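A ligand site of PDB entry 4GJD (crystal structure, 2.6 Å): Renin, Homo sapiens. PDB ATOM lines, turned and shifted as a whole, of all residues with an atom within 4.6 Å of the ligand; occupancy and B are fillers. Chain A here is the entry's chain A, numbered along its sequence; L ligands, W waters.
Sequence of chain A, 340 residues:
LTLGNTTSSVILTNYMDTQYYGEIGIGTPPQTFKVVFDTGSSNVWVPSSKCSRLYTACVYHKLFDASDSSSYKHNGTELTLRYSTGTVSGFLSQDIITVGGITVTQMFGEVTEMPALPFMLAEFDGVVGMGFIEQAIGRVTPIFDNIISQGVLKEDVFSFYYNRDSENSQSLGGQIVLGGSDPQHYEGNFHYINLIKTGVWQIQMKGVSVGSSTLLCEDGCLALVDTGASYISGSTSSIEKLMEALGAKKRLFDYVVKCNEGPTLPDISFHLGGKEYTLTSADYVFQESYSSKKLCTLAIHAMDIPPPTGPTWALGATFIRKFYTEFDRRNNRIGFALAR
OD2 of Asp 226 is in salt-bridge range of N1 of the ligand (2.8 Å). A nitrogen (N1) of the ligand lies within salt-bridge range of the side-chain carboxylate (OD1) of Asp 38, at 2.8 Å. N of Ser 84 lies within hydrogen-bond range of O3 of the ligand, 3.1 Å away. The side-chain hydroxyl (OG) of Ser 84 sits at hydrogen-bond distance from an oxygen (O3) of the ligand (3.3 Å). The backbone NH (N) of Tyr 20 is in hydrogen-bond range of an oxygen (O5) of the ligand, at 3.2 Å. The backbone carbonyl oxygen of Gly 228 sits close to a nitrogen (N3) of the ligand (3.2 Å). The side-chain hydroxyl (OG1) of Thr 85 sits at hydrogen-bond distance from an oxygen (O4) of the ligand, 3.2 Å away.
O of Thr 18 touches C30 of the ligand, at 3.5 Å. CA of Gln 19 touches C30 of the ligand (3.7 Å). Val 36 touches the ligand. Gly 40 touches the ligand (O to C1, 3.4 Å). Tyr 83 touches the ligand (CB to O3, 3.2 Å). Pro 118 touches the ligand. CE1 of Phe 119 touches O4 of the ligand (3.9 Å). Phe 124 touches the ligand. Val 127 touches the ligand (CG2 to C19, 3.3 Å). Tyr 162 touches the ligand. Thr 227 touches the ligand. Ala 229 touches the ligand. Ile 305 touches the ligand. Pro 306 touches the ligand. Within 4 Å of the ligand: Thr 18, Gln 19, Tyr 20, Val 36, Asp 38, Gly 40, Tyr 83, Ser 84, Thr 85, Pro 118, Phe 119, Phe 124, Val 127, Tyr 162, Asp 226, Thr 227, Gly 228, Ala 229, Ile 305 and Pro 306.
OD1 of Asp 38 lies close to OD1 of Asp 226 (2.7 Å). OD1 of Asp 226 sits at hydrogen-bond distance from N of Gly 228 (3.0 Å). OD1 of Asp 226 sits at hydrogen-bond distance from N of Gly 40, 3.2 Å away. N of Gly 40 sits at hydrogen-bond distance from OD1 of Asp 38 (3.1 Å). The side-chain carboxylate (OD2) of Asp 38 sits at hydrogen-bond distance from the side-chain hydroxyl (OG) of Ser 41, at 2.6 Å. O of Ala 229 is in hydrogen-bond range of N of Ala 317 (2.9 Å). O of Thr 18 sits at hydrogen-bond distance from OG of Ser 230 (2.6 Å). The backbone carbonyl oxygen (O) of Leu 121 lies within hydrogen-bond range of the side-chain amide nitrogen (NE2) of Gln 19.
Water W3 bridges a nitrogen (N2) of the ligand (2.9 Å) and the backbone carbonyl oxygen of Arg 82 (2.9 Å). Water W2 lies within hydrogen-bond range of O of Gly 40 (2.9 Å) and O1 of the ligand (3.2 Å).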
ATOM      1  N   THR A  18      -6.496 -18.414  -7.632  1.00  0.00           N
ATOM      2  CA  THR A  18      -5.260 -18.245  -8.390  1.00  0.00           C
ATOM      3  C   THR A  18      -3.988 -18.605  -7.635  1.00  0.00           C
ATOM      4  O   THR A  18      -2.993 -18.925  -8.287  1.00  0.00           O
ATOM      5  CB  THR A  18      -5.144 -16.868  -9.071  1.00  0.00           C
ATOM      6  OG1 THR A  18      -5.304 -15.816  -8.107  1.00  0.00           O
ATOM      7  CG2 THR A  18      -6.079 -16.716 -10.234  1.00  0.00           C
ATOM      8  N   GLN A  19      -3.985 -18.493  -6.288  1.00  0.00           N
ATOM      9  CA  GLN A  19      -2.779 -18.833  -5.497  1.00  0.00           C
ATOM     10  C   GLN A  19      -3.144 -19.754  -4.367  1.00  0.00           C
ATOM     11  O   GLN A  19      -4.035 -19.442  -3.605  1.00  0.00           O
ATOM     12  CB  GLN A  19      -2.072 -17.585  -4.957  1.00  0.00           C
ATOM     13  CG  GLN A  19      -1.639 -16.573  -6.049  1.00  0.00           C
ATOM     14  CD  GLN A  19      -1.100 -15.286  -5.494  1.00  0.00           C
ATOM     15  OE1 GLN A  19      -0.559 -15.247  -4.391  1.00  0.00           O
ATOM     16  NE2 GLN A  19      -1.238 -14.192  -6.241  1.00  0.00           N
ATOM     17  N   TYR A  20      -2.460 -20.909  -4.270  1.00  0.00           N
ATOM     18  CA  TYR A  20      -2.671 -21.901  -3.213  1.00  0.00           C
ATOM     19  C   TYR A  20      -1.348 -22.066  -2.537  1.00  0.00           C
ATOM     20  O   TYR A  20      -0.353 -22.400  -3.188  1.00  0.00           O
ATOM     21  CB  TYR A  20      -3.159 -23.240  -3.770  1.00  0.00           C
ATOM     22  CG  TYR A  20      -4.544 -23.210  -4.395  1.00  0.00           C
ATOM     23  CD1 TYR A  20      -4.741 -22.738  -5.681  1.00  0.00           C
ATOM     24  CD2 TYR A  20      -5.646 -23.735  -3.718  1.00  0.00           C
ATOM     25  CE1 TYR A  20      -6.001 -22.725  -6.268  1.00  0.00           C
ATOM     26  CE2 TYR A  20      -6.912 -23.772  -4.303  1.00  0.00           C
ATOM     27  CZ  TYR A  20      -7.074 -23.273  -5.591  1.00  0.00           C
ATOM     28  OH  TYR A  20      -8.298 -23.301  -6.208  1.00  0.00           O
ATOM     29  N   VAL A  36       4.303 -21.729  -1.950  1.00  0.00           N
ATOM     30  CA  VAL A  36       3.632 -22.454  -3.020  1.00  0.00           C
ATOM     31  C   VAL A  36       4.375 -23.800  -3.194  1.00  0.00           C
ATOM     32  O   VAL A  36       5.611 -23.822  -3.304  1.00  0.00           O
ATOM     33  CB  VAL A  36       3.607 -21.633  -4.340  1.00  0.00           C
ATOM     34  CG1 VAL A  36       3.132 -22.484  -5.518  1.00  0.00           C
ATOM     35  CG2 VAL A  36       2.715 -20.402  -4.189  1.00  0.00           C
ATOM     36  N   ASP A  38       5.164 -26.429  -5.580  1.00  0.00           N
ATOM     37  CA  ASP A  38       5.284 -26.419  -7.055  1.00  0.00           C
ATOM     38  C   ASP A  38       5.876 -27.671  -7.672  1.00  0.00           C
ATOM     39  O   ASP A  38       7.076 -27.881  -7.562  1.00  0.00           O
ATOM     40  CB  ASP A  38       6.118 -25.162  -7.457  1.00  0.00           C
ATOM     41  CG  ASP A  38       6.212 -24.830  -8.927  1.00  0.00           C
ATOM     42  OD1 ASP A  38       5.368 -25.301  -9.699  1.00  0.00           O
ATOM     43  OD2 ASP A  38       7.099 -24.026  -9.292  1.00  0.00           O
ATOM     44  N   GLY A  40       6.140 -28.062 -10.845  1.00  0.00           N
ATOM     45  CA  GLY A  40       6.788 -27.535 -12.048  1.00  0.00           C
ATOM     46  C   GLY A  40       8.194 -26.994 -11.857  1.00  0.00           C
ATOM     47  O   GLY A  40       8.767 -26.487 -12.822  1.00  0.00           O
ATOM     48  N   SER A  41       8.756 -27.108 -10.623  1.00  0.00           N
ATOM     49  CA  SER A  41      10.117 -26.653 -10.249  1.00  0.00           C
ATOM     50  C   SER A  41      10.669 -27.472  -9.051  1.00  0.00           C
ATOM     51  O   SER A  41       9.919 -28.200  -8.398  1.00  0.00           O
ATOM     52  CB  SER A  41      10.177 -25.146 -10.006  1.00  0.00           C
ATOM     53  OG  SER A  41       9.536 -24.751  -8.802  1.00  0.00           O
ATOM     54  N   ARG A  82      14.120 -18.888 -12.615  1.00  0.00           N
ATOM     55  CA  ARG A  82      13.198 -18.341 -13.612  1.00  0.00           C
ATOM     56  C   ARG A  82      11.849 -19.022 -13.581  1.00  0.00           C
ATOM     57  O   ARG A  82      11.771 -20.249 -13.524  1.00  0.00           O
ATOM     58  CB  ARG A  82      13.833 -18.407 -15.014  1.00  0.00           C
ATOM     59  CG  ARG A  82      14.961 -17.393 -15.183  1.00  0.00           C
ATOM     60  CD  ARG A  82      15.834 -17.614 -16.397  1.00  0.00           C
ATOM     61  NE  ARG A  82      17.091 -16.863 -16.307  1.00  0.00           N
ATOM     62  CZ  ARG A  82      18.222 -17.330 -15.762  1.00  0.00           C
ATOM     63  NH1 ARG A  82      18.249 -18.556 -15.249  1.00  0.00           N
ATOM     64  NH2 ARG A  82      19.301 -16.575 -15.709  1.00  0.00           N
ATOM     65  N   TYR A  83      10.788 -18.200 -13.601  1.00  0.00           N
ATOM     66  CA  TYR A  83       9.395 -18.637 -13.567  1.00  0.00           C
ATOM     67  C   TYR A  83       8.626 -18.033 -14.747  1.00  0.00           C
ATOM     68  O   TYR A  83       9.234 -17.372 -15.580  1.00  0.00           O
ATOM     69  CB  TYR A  83       8.780 -18.324 -12.189  1.00  0.00           C
ATOM     70  CG  TYR A  83       9.510 -19.053 -11.083  1.00  0.00           C
ATOM     71  CD1 TYR A  83       9.398 -20.438 -10.938  1.00  0.00           C
ATOM     72  CD2 TYR A  83      10.370 -18.377 -10.228  1.00  0.00           C
ATOM     73  CE1 TYR A  83      10.099 -21.124  -9.939  1.00  0.00           C
ATOM     74  CE2 TYR A  83      11.083 -19.057  -9.234  1.00  0.00           C
ATOM     75  CZ  TYR A  83      10.942 -20.429  -9.100  1.00  0.00           C
ATOM     76  OH  TYR A  83      11.640 -21.121  -8.141  1.00  0.00           O
ATOM     77  N   SER A  84       7.323 -18.278 -14.853  1.00  0.00           N
ATOM     78  CA  SER A  84       6.576 -17.801 -16.021  1.00  0.00           C
ATOM     79  C   SER A  84       6.439 -16.308 -16.137  1.00  0.00           C
ATOM     80  O   SER A  84       6.487 -15.747 -17.230  1.00  0.00           O
ATOM     81  CB  SER A  84       5.211 -18.480 -16.119  1.00  0.00           C
ATOM     82  OG  SER A  84       4.322 -17.985 -15.140  1.00  0.00           O
ATOM     83  N   THR A  85       6.207 -15.689 -14.967  1.00  0.00           N
ATOM     84  CA  THR A  85       5.869 -14.294 -14.661  1.00  0.00           C
ATOM     85  C   THR A  85       7.052 -13.377 -14.218  1.00  0.00           C
ATOM     86  O   THR A  85       6.890 -12.147 -14.234  1.00  0.00           O
ATOM     87  CB  THR A  85       4.806 -14.315 -13.507  1.00  0.00           C
ATOM     88  OG1 THR A  85       5.390 -14.964 -12.362  1.00  0.00           O
ATOM     89  CG2 THR A  85       3.499 -15.041 -13.872  1.00  0.00           C
ATOM     90  N   PRO A 118       6.420  -9.557 -10.818  1.00  0.00           N
ATOM     91  CA  PRO A 118       5.083  -9.840 -10.263  1.00  0.00           C
ATOM     92  C   PRO A 118       4.959 -10.028  -8.737  1.00  0.00           C
ATOM     93  O   PRO A 118       3.846 -10.173  -8.245  1.00  0.00           O
ATOM     94  CB  PRO A 118       4.747 -11.166 -10.959  1.00  0.00           C
ATOM     95  CG  PRO A 118       6.089 -11.891 -10.977  1.00  0.00           C
ATOM     96  CD  PRO A 118       7.146 -10.821 -11.121  1.00  0.00           C
ATOM     97  N   PHE A 119       6.084 -10.068  -8.007  1.00  0.00           N
ATOM     98  CA  PHE A 119       6.109 -10.374  -6.589  1.00  0.00           C
ATOM     99  C   PHE A 119       5.295  -9.499  -5.638  1.00  0.00           C
ATOM    100  O   PHE A 119       5.016  -9.932  -4.530  1.00  0.00           O
ATOM    101  CB  PHE A 119       7.528 -10.735  -6.116  1.00  0.00           C
ATOM    102  CG  PHE A 119       8.084 -11.900  -6.929  1.00  0.00           C
ATOM    103  CD1 PHE A 119       7.600 -13.200  -6.731  1.00  0.00           C
ATOM    104  CD2 PHE A 119       8.987 -11.680  -7.959  1.00  0.00           C
ATOM    105  CE1 PHE A 119       8.036 -14.257  -7.554  1.00  0.00           C
ATOM    106  CE2 PHE A 119       9.423 -12.738  -8.781  1.00  0.00           C
ATOM    107  CZ  PHE A 119       8.944 -14.021  -8.569  1.00  0.00           C
ATOM    108  N   LEU A 121       2.155  -8.877  -6.320  1.00  0.00           N
ATOM    109  CA  LEU A 121       0.887  -9.585  -6.517  1.00  0.00           C
ATOM    110  C   LEU A 121       0.882 -10.884  -5.722  1.00  0.00           C
ATOM    111  O   LEU A 121      -0.171 -11.535  -5.602  1.00  0.00           O
ATOM    112  CB  LEU A 121       0.684  -9.998  -7.986  1.00  0.00           C
ATOM    113  CG  LEU A 121       0.768  -8.975  -9.137  1.00  0.00           C
ATOM    114  CD1 LEU A 121       0.829  -9.718 -10.487  1.00  0.00           C
ATOM    115  CD2 LEU A 121      -0.381  -7.942  -9.093  1.00  0.00           C
ATOM    116  N   ALA A 122       2.070 -11.324  -5.277  1.00  0.00           N
ATOM    117  CA  ALA A 122       2.213 -12.576  -4.540  1.00  0.00           C
ATOM    118  C   ALA A 122       1.721 -12.453  -3.123  1.00  0.00           C
ATOM    119  O   ALA A 122       2.149 -11.586  -2.384  1.00  0.00           O
ATOM    120  CB  ALA A 122       3.661 -13.069  -4.574  1.00  0.00           C
ATOM    121  N   PHE A 124       1.910 -15.199  -1.262  1.00  0.00           N
ATOM    122  CA  PHE A 124       2.896 -16.121  -0.669  1.00  0.00           C
ATOM    123  C   PHE A 124       4.281 -15.436  -0.621  1.00  0.00           C
ATOM    124  O   PHE A 124       4.543 -14.528  -1.420  1.00  0.00           O
ATOM    125  CB  PHE A 124       2.955 -17.418  -1.508  1.00  0.00           C
ATOM    126  CG  PHE A 124       3.301 -17.173  -2.969  1.00  0.00           C
ATOM    127  CD1 PHE A 124       2.321 -16.828  -3.890  1.00  0.00           C
ATOM    128  CD2 PHE A 124       4.624 -17.246  -3.415  1.00  0.00           C
ATOM    129  CE1 PHE A 124       2.645 -16.580  -5.229  1.00  0.00           C
ATOM    130  CE2 PHE A 124       4.953 -16.962  -4.754  1.00  0.00           C
ATOM    131  CZ  PHE A 124       3.960 -16.670  -5.651  1.00  0.00           C
ATOM    132  N   VAL A 127       8.657 -20.333  -2.428  1.00  0.00           N
ATOM    133  CA  VAL A 127       8.304 -21.515  -3.213  1.00  0.00           C
ATOM    134  C   VAL A 127       9.030 -22.720  -2.677  1.00  0.00           C
ATOM    135  O   VAL A 127      10.204 -22.631  -2.328  1.00  0.00           O
ATOM    136  CB  VAL A 127       8.665 -21.286  -4.725  1.00  0.00           C
ATOM    137  CG1 VAL A 127       8.493 -22.551  -5.571  1.00  0.00           C
ATOM    138  CG2 VAL A 127       7.872 -20.109  -5.321  1.00  0.00           C
ATOM    139  N   TYR A 162      -7.152 -29.110  -4.269  1.00  0.00           N
ATOM    140  CA  TYR A 162      -7.347 -27.666  -4.385  1.00  0.00           C
ATOM    141  C   TYR A 162      -8.827 -27.452  -4.356  1.00  0.00           C
ATOM    142  O   TYR A 162      -9.528 -27.967  -5.214  1.00  0.00           O
ATOM    143  CB  TYR A 162      -6.744 -27.105  -5.707  1.00  0.00           C
ATOM    144  CG  TYR A 162      -5.250 -26.846  -5.722  1.00  0.00           C
ATOM    145  CD1 TYR A 162      -4.471 -27.033  -4.574  1.00  0.00           C
ATOM    146  CD2 TYR A 162      -4.610 -26.411  -6.879  1.00  0.00           C
ATOM    147  CE1 TYR A 162      -3.091 -26.801  -4.599  1.00  0.00           C
ATOM    148  CE2 TYR A 162      -3.231 -26.189  -6.915  1.00  0.00           C
ATOM    149  CZ  TYR A 162      -2.486 -26.362  -5.771  1.00  0.00           C
ATOM    150  OH  TYR A 162      -1.135 -26.109  -5.797  1.00  0.00           O
ATOM    151  N   LEU A 224       2.353 -30.907 -18.900  1.00  0.00           N
ATOM    152  CA  LEU A 224       3.049 -30.717 -17.622  1.00  0.00           C
ATOM    153  C   LEU A 224       1.950 -30.547 -16.539  1.00  0.00           C
ATOM    154  O   LEU A 224       1.051 -29.711 -16.690  1.00  0.00           O
ATOM    155  CB  LEU A 224       3.982 -29.492 -17.696  1.00  0.00           C
ATOM    156  CG  LEU A 224       4.818 -29.199 -16.438  1.00  0.00           C
ATOM    157  CD1 LEU A 224       5.994 -30.157 -16.306  1.00  0.00           C
ATOM    158  CD2 LEU A 224       5.288 -27.777 -16.436  1.00  0.00           C
ATOM    159  N   ASP A 226       1.314 -29.159 -13.395  1.00  0.00           N
ATOM    160  CA  ASP A 226       1.913 -28.103 -12.564  1.00  0.00           C
ATOM    161  C   ASP A 226       1.013 -27.548 -11.463  1.00  0.00           C
ATOM    162  O   ASP A 226       0.120 -26.758 -11.730  1.00  0.00           O
ATOM    163  CB  ASP A 226       2.442 -26.975 -13.482  1.00  0.00           C
ATOM    164  CG  ASP A 226       3.338 -25.963 -12.819  1.00  0.00           C
ATOM    165  OD1 ASP A 226       3.664 -26.135 -11.621  1.00  0.00           O
ATOM    166  OD2 ASP A 226       3.756 -24.998 -13.504  1.00  0.00           O
ATOM    167  N   THR A 227       1.340 -27.905 -10.208  1.00  0.00           N
ATOM    168  CA  THR A 227       0.614 -27.454  -9.017  1.00  0.00           C
ATOM    169  C   THR A 227       0.918 -25.976  -8.704  1.00  0.00           C
ATOM    170  O   THR A 227       0.165 -25.333  -7.964  1.00  0.00           O
ATOM    171  CB  THR A 227       0.928 -28.361  -7.814  1.00  0.00           C
ATOM    172  OG1 THR A 227       2.338 -28.340  -7.563  1.00  0.00           O
ATOM    173  CG2 THR A 227       0.458 -29.794  -8.034  1.00  0.00           C
ATOM    174  N   GLY A 228       2.020 -25.467  -9.251  1.00  0.00           N
ATOM    175  CA  GLY A 228       2.446 -24.079  -9.096  1.00  0.00           C
ATOM    176  C   GLY A 228       1.907 -23.171 -10.182  1.00  0.00           C
ATOM    177  O   GLY A 228       2.236 -21.984 -10.189  1.00  0.00           O
ATOM    178  N   ALA A 229       1.074 -23.704 -11.077  1.00  0.00           N
ATOM    179  CA  ALA A 229       0.453 -22.937 -12.154  1.00  0.00           C
ATOM    180  C   ALA A 229      -0.994 -22.666 -11.736  1.00  0.00           C
ATOM    181  O   ALA A 229      -1.659 -23.547 -11.184  1.00  0.00           O
ATOM    182  CB  ALA A 229       0.494 -23.718 -13.475  1.00  0.00           C
ATOM    183  N   SER A 230      -1.472 -21.456 -12.012  1.00  0.00           N
ATOM    184  CA  SER A 230      -2.820 -21.035 -11.681  1.00  0.00           C
ATOM    185  C   SER A 230      -3.854 -21.576 -12.606  1.00  0.00           C
ATOM    186  O   SER A 230      -4.959 -21.845 -12.177  1.00  0.00           O
ATOM    187  CB  SER A 230      -2.930 -19.520 -11.650  1.00  0.00           C
ATOM    188  OG  SER A 230      -2.004 -18.930 -10.742  1.00  0.00           O
ATOM    189  N   ASP A 304       3.989 -19.816 -23.401  1.00  0.00           N
ATOM    190  CA  ASP A 304       5.006 -20.453 -24.216  1.00  0.00           C
ATOM    191  C   ASP A 304       6.130 -20.879 -23.297  1.00  0.00           C
ATOM    192  O   ASP A 304       6.978 -20.067 -22.884  1.00  0.00           O
ATOM    193  CB  ASP A 304       5.432 -19.599 -25.417  1.00  0.00           C
ATOM    194  CG  ASP A 304       4.273 -19.279 -26.334  1.00  0.00           C
ATOM    195  OD1 ASP A 304       3.827 -18.116 -26.346  1.00  0.00           O
ATOM    196  OD2 ASP A 304       3.771 -20.205 -26.994  1.00  0.00           O
ATOM    197  N   ILE A 305       6.063 -22.153 -22.877  1.00  0.00           N
ATOM    198  CA  ILE A 305       7.025 -22.788 -21.988  1.00  0.00           C
ATOM    199  C   ILE A 305       8.232 -23.177 -22.848  1.00  0.00           C
ATOM    200  O   ILE A 305       8.061 -23.891 -23.833  1.00  0.00           O
ATOM    201  CB  ILE A 305       6.390 -23.952 -21.174  1.00  0.00           C
ATOM    202  CG1 ILE A 305       5.279 -23.395 -20.228  1.00  0.00           C
ATOM    203  CG2 ILE A 305       7.454 -24.740 -20.386  1.00  0.00           C
ATOM    204  CD1 ILE A 305       4.162 -24.332 -19.920  1.00  0.00           C
ATOM    205  N   PRO A 306       9.420 -22.605 -22.565  1.00  0.00           N
ATOM    206  CA  PRO A 306      10.604 -22.854 -23.400  1.00  0.00           C
ATOM    207  C   PRO A 306      11.183 -24.267 -23.320  1.00  0.00           C
ATOM    208  O   PRO A 306      10.908 -24.963 -22.347  1.00  0.00           O
ATOM    209  CB  PRO A 306      11.616 -21.829 -22.879  1.00  0.00           C
ATOM    210  CG  PRO A 306      11.235 -21.615 -21.466  1.00  0.00           C
ATOM    211  CD  PRO A 306       9.737 -21.668 -21.461  1.00  0.00           C
ATOM    212  N   ALA A 317      -4.097 -25.176 -11.503  1.00  0.00           N
ATOM    213  CA  ALA A 317      -5.199 -25.214 -10.518  1.00  0.00           C
ATOM    214  C   ALA A 317      -6.610 -25.327 -11.103  1.00  0.00           C
ATOM    215  O   ALA A 317      -7.527 -25.834 -10.423  1.00  0.00           O
ATOM    216  CB  ALA A 317      -5.110 -24.036  -9.543  1.00  0.00           C
HETATM  217  C1  LIG L   1       6.791 -23.750 -12.702  1.00  0.00           C
HETATM  218  C2  LIG L   1       6.558 -23.014 -14.045  1.00  0.00           C
HETATM  219  C3  LIG L   1       6.161 -21.530 -13.813  1.00  0.00           C
HETATM  220  C4  LIG L   1       4.952 -21.338 -12.834  1.00  0.00           C
HETATM  221  C5  LIG L   1       5.159 -22.228 -11.577  1.00  0.00           C
HETATM  222  N1  LIG L   1       5.562 -23.621 -11.909  1.00  0.00           N
HETATM  223  N2  LIG L   1       7.722 -23.103 -14.909  1.00  0.00           N
HETATM  224  C6  LIG L   1       4.733 -19.907 -12.362  1.00  0.00           C
HETATM  225  S1  LIG L   1       7.585 -23.424 -16.521  1.00  0.00           S
HETATM  226  C7  LIG L   1       8.136 -21.882 -17.206  1.00  0.00           C
HETATM  227  O1  LIG L   1       8.549 -24.486 -16.784  1.00  0.00           O
HETATM  228  O2  LIG L   1       6.192 -23.622 -16.911  1.00  0.00           O
HETATM  229  C8  LIG L   1       9.419 -21.403 -16.871  1.00  0.00           C
HETATM  230  C9  LIG L   1       9.885 -20.190 -17.416  1.00  0.00           C
HETATM  231  C10 LIG L   1       9.079 -19.454 -18.287  1.00  0.00           C
HETATM  232  C11 LIG L   1       7.798 -19.937 -18.646  1.00  0.00           C
HETATM  233  C12 LIG L   1       7.314 -21.141 -18.091  1.00  0.00           C
HETATM  234  C13 LIG L   1       9.611 -18.127 -18.875  1.00  0.00           C
HETATM  235  O3  LIG L   1       5.672 -19.132 -12.385  1.00  0.00           O
HETATM  236  N3  LIG L   1       3.499 -19.539 -11.893  1.00  0.00           N
HETATM  237  C14 LIG L   1       3.160 -18.209 -11.346  1.00  0.00           C
HETATM  238  C15 LIG L   1       3.135 -18.121  -9.774  1.00  0.00           C
HETATM  239  O4  LIG L   1       5.437 -16.460  -9.503  1.00  0.00           O
HETATM  240  C16 LIG L   1       4.490 -18.686  -9.240  1.00  0.00           C
HETATM  241  C17 LIG L   1       5.595 -17.812  -9.200  1.00  0.00           C
HETATM  242  C18 LIG L   1       6.872 -18.269  -8.811  1.00  0.00           C
HETATM  243  C19 LIG L   1       7.070 -19.627  -8.501  1.00  0.00           C
HETATM  244  C20 LIG L   1       5.994 -20.537  -8.539  1.00  0.00           C
HETATM  245  C21 LIG L   1       4.727 -20.048  -8.900  1.00  0.00           C
HETATM  246  C22 LIG L   1       4.207 -15.841  -9.315  1.00  0.00           C
HETATM  247  C23 LIG L   1       3.016 -16.598  -9.443  1.00  0.00           C
HETATM  248  C24 LIG L   1       1.787 -15.877  -9.245  1.00  0.00           C
HETATM  249  C25 LIG L   1       1.750 -14.495  -8.943  1.00  0.00           C
HETATM  250  C26 LIG L   1       2.957 -13.777  -8.784  1.00  0.00           C
HETATM  251  C27 LIG L   1       4.174 -14.467  -8.970  1.00  0.00           C
HETATM  252  C28 LIG L   1       1.887 -18.923  -9.245  1.00  0.00           C
HETATM  253  C29 LIG L   1       1.688 -19.124  -7.713  1.00  0.00           C
HETATM  254  C30 LIG L   1       0.290 -19.711  -7.388  1.00  0.00           C
HETATM  255  C31 LIG L   1       0.240 -21.255  -7.592  1.00  0.00           C
HETATM  256  O5  LIG L   1      -0.957 -21.775  -6.978  1.00  0.00           O
HETATM  257  C32 LIG L   1      -1.724 -22.605  -7.851  1.00  0.00           C
HETATM  258  O   HOH W   1       2.673 -20.565 -15.223  1.00  0.00           O
HETATM  259  O   HOH W   2       9.160 -27.355 -15.521  1.00  0.00           O
HETATM  260  O   HOH W   3      10.256 -22.779 -13.496  1.00  0.00           O
